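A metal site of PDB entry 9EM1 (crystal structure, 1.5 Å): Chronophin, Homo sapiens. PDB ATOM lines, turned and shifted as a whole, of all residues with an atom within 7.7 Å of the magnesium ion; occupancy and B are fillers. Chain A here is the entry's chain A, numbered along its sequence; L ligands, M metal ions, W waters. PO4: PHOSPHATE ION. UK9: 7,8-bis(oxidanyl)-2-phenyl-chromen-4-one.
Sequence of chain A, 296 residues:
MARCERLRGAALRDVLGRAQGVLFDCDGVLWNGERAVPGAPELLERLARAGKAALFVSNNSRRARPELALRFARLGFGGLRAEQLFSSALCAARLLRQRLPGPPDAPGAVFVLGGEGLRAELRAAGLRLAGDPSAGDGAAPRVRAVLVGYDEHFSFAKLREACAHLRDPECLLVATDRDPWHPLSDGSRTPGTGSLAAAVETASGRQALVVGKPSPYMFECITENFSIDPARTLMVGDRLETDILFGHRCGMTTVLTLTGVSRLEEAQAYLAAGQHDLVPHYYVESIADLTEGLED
Of the 22 residues printed, 3 come within 4 Å of the magnesium ion.
The side-chain amino group (NZ) of Lys 213 lies within salt-bridge range of the side-chain carboxylate (OD1) of Asp 25. NE1 of Trp 31 is in hydrogen-bond range of OD1 of Asp 27. The backbone NH (N) of Asp 238 is in hydrogen-bond range of the side-chain carboxylate (OD2) of Asp 243 (3.2 Å). The backbone NH (N) of Val 261 sits at hydrogen-bond distance from the side-chain carboxylate (OD2) of Asp 238, 2.9 Å away. O of Val 236 sits at hydrogen-bond distance from N of Asp 25 (2.9 Å).
The magnesium ion is bound by O4 of PO4 L1 (2.0 Å), OD2 of Asp 25 (2.0 Å), water W2 (2.0 Å), OD1 of Asp 238 (2.1 Å), water W1 (2.1 Å) and O of Asp 27 (2.2 Å).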
ATOM      1  N   ASP A  25       2.085  -6.549 -10.979  1.00  0.00           N
ATOM      2  CA  ASP A  25       2.698  -5.343 -11.486  1.00  0.00           C
ATOM      3  C   ASP A  25       3.849  -4.978 -10.555  1.00  0.00           C
ATOM      4  O   ASP A  25       3.901  -5.378  -9.390  1.00  0.00           O
ATOM      5  CB  ASP A  25       1.678  -4.219 -11.542  1.00  0.00           C
ATOM      6  CG  ASP A  25       2.304  -2.921 -11.980  1.00  0.00           C
ATOM      7  OD1 ASP A  25       2.982  -2.952 -13.011  1.00  0.00           O
ATOM      8  OD2 ASP A  25       2.117  -1.936 -11.297  1.00  0.00           O
ATOM      9  N   CYS A  26       4.779  -4.187 -11.066  1.00  0.00           N
ATOM     10  CA  CYS A  26       5.974  -3.813 -10.315  1.00  0.00           C
ATOM     11  C   CYS A  26       5.929  -2.427  -9.682  1.00  0.00           C
ATOM     12  O   CYS A  26       5.852  -2.290  -8.444  1.00  0.00           O
ATOM     13  CB  CYS A  26       7.197  -3.944 -11.275  1.00  0.00           C
ATOM     14  SG  CYS A  26       7.461  -5.625 -11.811  1.00  0.00           S
ATOM     15  N   ASP A  27       6.000  -1.363 -10.492  1.00  0.00           N
ATOM     16  CA  ASP A  27       6.047  -0.022  -9.943  1.00  0.00           C
ATOM     17  C   ASP A  27       4.709   0.304  -9.245  1.00  0.00           C
ATOM     18  O   ASP A  27       3.619   0.123  -9.825  1.00  0.00           O
ATOM     19  CB  ASP A  27       6.332   1.037 -11.024  1.00  0.00           C
ATOM     20  CG  ASP A  27       7.578   0.762 -11.858  1.00  0.00           C
ATOM     21  OD1 ASP A  27       8.543   0.157 -11.361  1.00  0.00           O
ATOM     22  OD2 ASP A  27       7.608   1.185 -13.025  1.00  0.00           O
ATOM     23  N   GLY A  28       4.788   0.773  -8.016  1.00  0.00           N
ATOM     24  CA  GLY A  28       3.623   1.101  -7.196  1.00  0.00           C
ATOM     25  C   GLY A  28       3.081  -0.071  -6.408  1.00  0.00           C
ATOM     26  O   GLY A  28       2.129   0.122  -5.652  1.00  0.00           O
ATOM     27  N   VAL A  29       3.647  -1.250  -6.570  1.00  0.00           N
ATOM     28  CA  VAL A  29       3.132  -2.509  -6.002  1.00  0.00           C
ATOM     29  C   VAL A  29       4.203  -3.138  -5.128  1.00  0.00           C
ATOM     30  O   VAL A  29       3.991  -3.384  -3.938  1.00  0.00           O
ATOM     31  CB  VAL A  29       2.719  -3.448  -7.124  1.00  0.00           C
ATOM     32  CG1 VAL A  29       2.304  -4.776  -6.570  1.00  0.00           C
ATOM     33  CG2 VAL A  29       1.572  -2.807  -7.933  1.00  0.00           C
ATOM     34  N   LEU A  30       5.364  -3.427  -5.716  1.00  0.00           N
ATOM     35  CA  LEU A  30       6.504  -3.972  -4.982  1.00  0.00           C
ATOM     36  C   LEU A  30       7.364  -2.902  -4.376  1.00  0.00           C
ATOM     37  O   LEU A  30       8.090  -3.159  -3.404  1.00  0.00           O
ATOM     38  CB  LEU A  30       7.380  -4.796  -5.927  1.00  0.00           C
ATOM     39  CG  LEU A  30       6.676  -5.893  -6.722  1.00  0.00           C
ATOM     40  CD1 LEU A  30       7.652  -6.502  -7.710  1.00  0.00           C
ATOM     41  CD2 LEU A  30       6.101  -6.939  -5.852  1.00  0.00           C
ATOM     42  N   TRP A  31       7.361  -1.708  -4.958  1.00  0.00           N
ATOM     43  CA  TRP A  31       8.229  -0.612  -4.601  1.00  0.00           C
ATOM     44  C   TRP A  31       7.631   0.695  -5.073  1.00  0.00           C
ATOM     45  O   TRP A  31       6.777   0.707  -5.978  1.00  0.00           O
ATOM     46  CB  TRP A  31       9.661  -0.765  -5.168  1.00  0.00           C
ATOM     47  CG  TRP A  31       9.735  -0.997  -6.678  1.00  0.00           C
ATOM     48  CD1 TRP A  31       9.403  -0.110  -7.650  1.00  0.00           C
ATOM     49  CD2 TRP A  31      10.172  -2.190  -7.351  1.00  0.00           C
ATOM     50  NE1 TRP A  31       9.544  -0.707  -8.902  1.00  0.00           N
ATOM     51  CE2 TRP A  31      10.018  -1.970  -8.738  1.00  0.00           C
ATOM     52  CE3 TRP A  31      10.648  -3.430  -6.910  1.00  0.00           C
ATOM     53  CZ2 TRP A  31      10.387  -2.922  -9.680  1.00  0.00           C
ATOM     54  CZ3 TRP A  31      10.987  -4.382  -7.857  1.00  0.00           C
ATOM     55  CH2 TRP A  31      10.863  -4.111  -9.222  1.00  0.00           C
ATOM     56  N   VAL A  57       5.001  -8.274 -14.307  1.00  0.00           N
ATOM     57  CA  VAL A  57       4.684  -7.596 -15.573  1.00  0.00           C
ATOM     58  C   VAL A  57       4.652  -6.092 -15.362  1.00  0.00           C
ATOM     59  O   VAL A  57       3.792  -5.579 -14.643  1.00  0.00           O
ATOM     60  CB  VAL A  57       3.326  -8.074 -16.135  1.00  0.00           C
ATOM     61  CG1 VAL A  57       2.225  -7.828 -15.138  1.00  0.00           C
ATOM     62  CG2 VAL A  57       3.024  -7.379 -17.436  1.00  0.00           C
ATOM     63  N   SER A  58       5.545  -5.373 -16.080  1.00  0.00           N
ATOM     64  CA  SER A  58       5.716  -3.942 -15.951  1.00  0.00           C
ATOM     65  C   SER A  58       5.666  -3.260 -17.306  1.00  0.00           C
ATOM     66  O   SER A  58       6.217  -3.769 -18.276  1.00  0.00           O
ATOM     67  CB  SER A  58       7.066  -3.688 -15.308  1.00  0.00           C
ATOM     68  OG  SER A  58       7.310  -2.326 -15.112  1.00  0.00           O
ATOM     69  N   ASN A  59       5.015  -2.083 -17.337  1.00  0.00           N
ATOM     70  CA  ASN A  59       5.053  -1.283 -18.568  1.00  0.00           C
ATOM     71  C   ASN A  59       6.297  -0.416 -18.649  1.00  0.00           C
ATOM     72  O   ASN A  59       6.501   0.293 -19.636  1.00  0.00           O
ATOM     73  CB  ASN A  59       3.810  -0.388 -18.669  1.00  0.00           C
ATOM     74  CG  ASN A  59       2.587  -1.133 -19.235  1.00  0.00           C
ATOM     75  OD1 ASN A  59       2.700  -2.251 -19.684  1.00  0.00           O
ATOM     76  ND2 ASN A  59       1.429  -0.491 -19.125  1.00  0.00           N
ATOM     77  N   ASP A 179       0.701   4.444 -20.698  1.00  0.00           N
ATOM     78  CA  ASP A 179       0.579   5.059 -19.376  1.00  0.00           C
ATOM     79  C   ASP A 179       0.840   6.582 -19.544  1.00  0.00           C
ATOM     80  O   ASP A 179       1.816   6.967 -20.178  1.00  0.00           O
ATOM     81  CB  ASP A 179       1.585   4.469 -18.367  1.00  0.00           C
ATOM     82  CG  ASP A 179       1.357   2.976 -18.050  1.00  0.00           C
ATOM     83  OD1 ASP A 179       0.477   2.370 -18.585  1.00  0.00           O
ATOM     84  OD2 ASP A 179       2.102   2.458 -17.218  1.00  0.00           O
ATOM     85  N   HIS A 182       3.868   9.247 -14.771  1.00  0.00           N
ATOM     86  CA  HIS A 182       4.306   8.444 -13.624  1.00  0.00           C
ATOM     87  C   HIS A 182       4.681   9.363 -12.479  1.00  0.00           C
ATOM     88  O   HIS A 182       5.235  10.447 -12.672  1.00  0.00           O
ATOM     89  CB  HIS A 182       5.481   7.584 -14.006  1.00  0.00           C
ATOM     90  CG  HIS A 182       5.184   6.675 -15.136  1.00  0.00           C
ATOM     91  ND1 HIS A 182       4.524   5.471 -14.974  1.00  0.00           N
ATOM     92  CD2 HIS A 182       5.398   6.824 -16.459  1.00  0.00           C
ATOM     93  CE1 HIS A 182       4.366   4.899 -16.154  1.00  0.00           C
ATOM     94  NE2 HIS A 182       4.906   5.697 -17.070  1.00  0.00           N
ATOM     95  N   LYS A 213       0.204  -3.665 -20.971  1.00  0.00           N
ATOM     96  CA  LYS A 213      -1.062  -3.589 -20.281  1.00  0.00           C
ATOM     97  C   LYS A 213      -1.704  -2.241 -20.590  1.00  0.00           C
ATOM     98  O   LYS A 213      -1.012  -1.226 -20.499  1.00  0.00           O
ATOM     99  CB  LYS A 213      -0.866  -3.659 -18.756  1.00  0.00           C
ATOM    100  CG  LYS A 213       0.005  -4.757 -18.251  1.00  0.00           C
ATOM    101  CD  LYS A 213       0.401  -4.549 -16.761  1.00  0.00           C
ATOM    102  CE  LYS A 213       1.503  -3.593 -16.555  1.00  0.00           C
ATOM    103  NZ  LYS A 213       1.612  -3.138 -15.166  1.00  0.00           N
ATOM    104  N   VAL A 236      -2.381  -8.472  -9.609  1.00  0.00           N
ATOM    105  CA  VAL A 236      -2.203  -7.489  -8.539  1.00  0.00           C
ATOM    106  C   VAL A 236      -1.550  -6.250  -9.122  1.00  0.00           C
ATOM    107  O   VAL A 236      -0.436  -6.315  -9.628  1.00  0.00           O
ATOM    108  CB  VAL A 236      -1.367  -8.065  -7.403  1.00  0.00           C
ATOM    109  CG1 VAL A 236      -1.248  -7.023  -6.261  1.00  0.00           C
ATOM    110  CG2 VAL A 236      -2.004  -9.337  -6.854  1.00  0.00           C
ATOM    111  N   GLY A 237      -2.247  -5.111  -9.066  1.00  0.00           N
ATOM    112  CA  GLY A 237      -1.729  -3.889  -9.634  1.00  0.00           C
ATOM    113  C   GLY A 237      -2.162  -2.653  -8.903  1.00  0.00           C
ATOM    114  O   GLY A 237      -3.034  -2.705  -8.029  1.00  0.00           O
ATOM    115  N   ASP A 238      -1.536  -1.529  -9.267  1.00  0.00           N
ATOM    116  CA  ASP A 238      -1.858  -0.256  -8.655  1.00  0.00           C
ATOM    117  C   ASP A 238      -2.607   0.708  -9.574  1.00  0.00           C
ATOM    118  O   ASP A 238      -2.973   1.809  -9.111  1.00  0.00           O
ATOM    119  CB  ASP A 238      -0.610   0.476  -8.119  1.00  0.00           C
ATOM    120  CG  ASP A 238       0.333   0.954  -9.226  1.00  0.00           C
ATOM    121  OD1 ASP A 238       0.727   0.127 -10.093  1.00  0.00           O
ATOM    122  OD2 ASP A 238       0.688   2.162  -9.235  1.00  0.00           O
ATOM    123  N   ARG A 239      -2.846   0.359 -10.832  1.00  0.00           N
ATOM    124  CA  ARG A 239      -3.385   1.327 -11.797  1.00  0.00           C
ATOM    125  C   ARG A 239      -4.640   0.765 -12.431  1.00  0.00           C
ATOM    126  O   ARG A 239      -4.612  -0.282 -13.097  1.00  0.00           O
ATOM    127  CB  ARG A 239      -2.310   1.685 -12.827  1.00  0.00           C
ATOM    128  CG  ARG A 239      -2.497   3.034 -13.432  1.00  0.00           C
ATOM    129  CD  ARG A 239      -1.219   3.488 -14.099  1.00  0.00           C
ATOM    130  NE  ARG A 239      -1.358   4.891 -14.509  1.00  0.00           N
ATOM    131  CZ  ARG A 239      -0.346   5.744 -14.618  1.00  0.00           C
ATOM    132  NH1 ARG A 239       0.913   5.341 -14.459  1.00  0.00           N
ATOM    133  NH2 ARG A 239      -0.624   7.038 -14.822  1.00  0.00           N
ATOM    134  N   THR A 242      -4.823   0.364 -16.365  1.00  0.00           N
ATOM    135  CA  THR A 242      -3.864  -0.516 -17.001  1.00  0.00           C
ATOM    136  C   THR A 242      -3.886  -1.899 -16.372  1.00  0.00           C
ATOM    137  O   THR A 242      -4.265  -2.858 -17.044  1.00  0.00           O
ATOM    138  CB  THR A 242      -2.472   0.104 -16.960  1.00  0.00           C
ATOM    139  OG1 THR A 242      -1.968   0.094 -15.623  1.00  0.00           O
ATOM    140  CG2 THR A 242      -2.505   1.567 -17.454  1.00  0.00           C
ATOM    141  N   ASP A 243      -3.588  -2.039 -15.076  1.00  0.00           N
ATOM    142  CA  ASP A 243      -3.527  -3.356 -14.461  1.00  0.00           C
ATOM    143  C   ASP A 243      -4.894  -3.988 -14.284  1.00  0.00           C
ATOM    144  O   ASP A 243      -5.075  -5.191 -14.569  1.00  0.00           O
ATOM    145  CB  ASP A 243      -2.849  -3.249 -13.089  1.00  0.00           C
ATOM    146  CG  ASP A 243      -1.520  -2.629 -13.179  1.00  0.00           C
ATOM    147  OD1 ASP A 243      -0.689  -3.076 -14.007  1.00  0.00           O
ATOM    148  OD2 ASP A 243      -1.280  -1.664 -12.422  1.00  0.00           O
ATOM    149  N   THR A 257      -3.890  -2.771  -5.214  1.00  0.00           N
ATOM    150  CA  THR A 257      -3.161  -2.320  -4.057  1.00  0.00           C
ATOM    151  C   THR A 257      -3.088  -0.793  -4.051  1.00  0.00           C
ATOM    152  O   THR A 257      -3.052  -0.174  -5.108  1.00  0.00           O
ATOM    153  CB  THR A 257      -1.759  -2.950  -3.989  1.00  0.00           C
ATOM    154  OG1 THR A 257      -1.129  -2.532  -2.765  1.00  0.00           O
ATOM    155  CG2 THR A 257      -0.887  -2.542  -5.180  1.00  0.00           C
ATOM    156  N   GLY A 260       0.192   2.752  -4.824  1.00  0.00           N
ATOM    157  CA  GLY A 260       0.609   3.353  -6.083  1.00  0.00           C
ATOM    158  C   GLY A 260      -0.292   4.452  -6.610  1.00  0.00           C
ATOM    159  O   GLY A 260      -0.733   5.355  -5.880  1.00  0.00           O
ATOM    160  N   VAL A 261      -0.534   4.396  -7.902  1.00  0.00           N
ATOM    161  CA  VAL A 261      -1.129   5.511  -8.640  1.00  0.00           C
ATOM    162  C   VAL A 261      -2.620   5.692  -8.325  1.00  0.00           C
ATOM    163  O   VAL A 261      -3.088   6.817  -8.085  1.00  0.00           O
ATOM    164  CB  VAL A 261      -0.890   5.318 -10.132  1.00  0.00           C
ATOM    165  CG1 VAL A 261      -1.769   6.315 -10.914  1.00  0.00           C
ATOM    166  CG2 VAL A 261       0.583   5.535 -10.469  1.00  0.00           C
HETATM  167  P   PO4 L   1       4.412  -0.409 -14.089  1.00  0.00           P
HETATM  168  O1  PO4 L   1       5.275  -1.461 -13.393  1.00  0.00           O
HETATM  169  O2  PO4 L   1       3.573  -1.057 -15.157  1.00  0.00           O
HETATM  170  O3  PO4 L   1       5.360   0.610 -14.785  1.00  0.00           O
HETATM  171  O4  PO4 L   1       3.557   0.250 -13.012  1.00  0.00           O
HETATM  172  C2  UK9 L   2       9.642   5.161 -15.996  1.00  0.00           C
HETATM  173  C4  UK9 L   2       9.518   6.553 -13.952  1.00  0.00           C
HETATM  174  C6  UK9 L   2       8.075   5.943 -12.132  1.00  0.00           C
HETATM  175  C7  UK9 L   2       7.618   4.865 -12.847  1.00  0.00           C
HETATM  176  C9  UK9 L   2      11.665   5.395 -17.245  1.00  0.00           C
HETATM  177  C11 UK9 L   2      13.741   5.682 -18.408  1.00  0.00           C
HETATM  178  C12 UK9 L   2      13.260   4.863 -19.441  1.00  0.00           C
HETATM  179  C13 UK9 L   2      11.997   4.321 -19.358  1.00  0.00           C
HETATM  180  C14 UK9 L   2      11.174   4.586 -18.260  1.00  0.00           C
HETATM  181  C   UK9 L   2       9.819   4.009 -18.151  1.00  0.00           C
HETATM  182  O   UK9 L   2       9.316   3.306 -19.050  1.00  0.00           O
HETATM  183  O1  UK9 L   2      10.902   5.681 -16.125  1.00  0.00           O
HETATM  184  O2  UK9 L   2      13.452   6.730 -16.313  1.00  0.00           O
HETATM  185  C1  UK9 L   2       9.105   4.364 -16.958  1.00  0.00           C
HETATM  186  C10 UK9 L   2      12.940   5.948 -17.299  1.00  0.00           C
HETATM  187  C3  UK9 L   2       9.065   5.460 -14.691  1.00  0.00           C
HETATM  188  C5  UK9 L   2       9.025   6.787 -12.684  1.00  0.00           C
HETATM  189  C8  UK9 L   2       8.107   4.618 -14.133  1.00  0.00           C
HETATM  190  O3  UK9 L   2      14.972   6.261 -18.461  1.00  0.00           O
HETATM  191 MG    MG M   1       2.220   0.086 -11.535  1.00  0.00          MG
HETATM  192  O   HOH W   1       2.201   2.213 -11.364  1.00  0.00           O
HETATM  193  O   HOH W   2       0.765  -0.038 -12.971  1.00  0.00           O
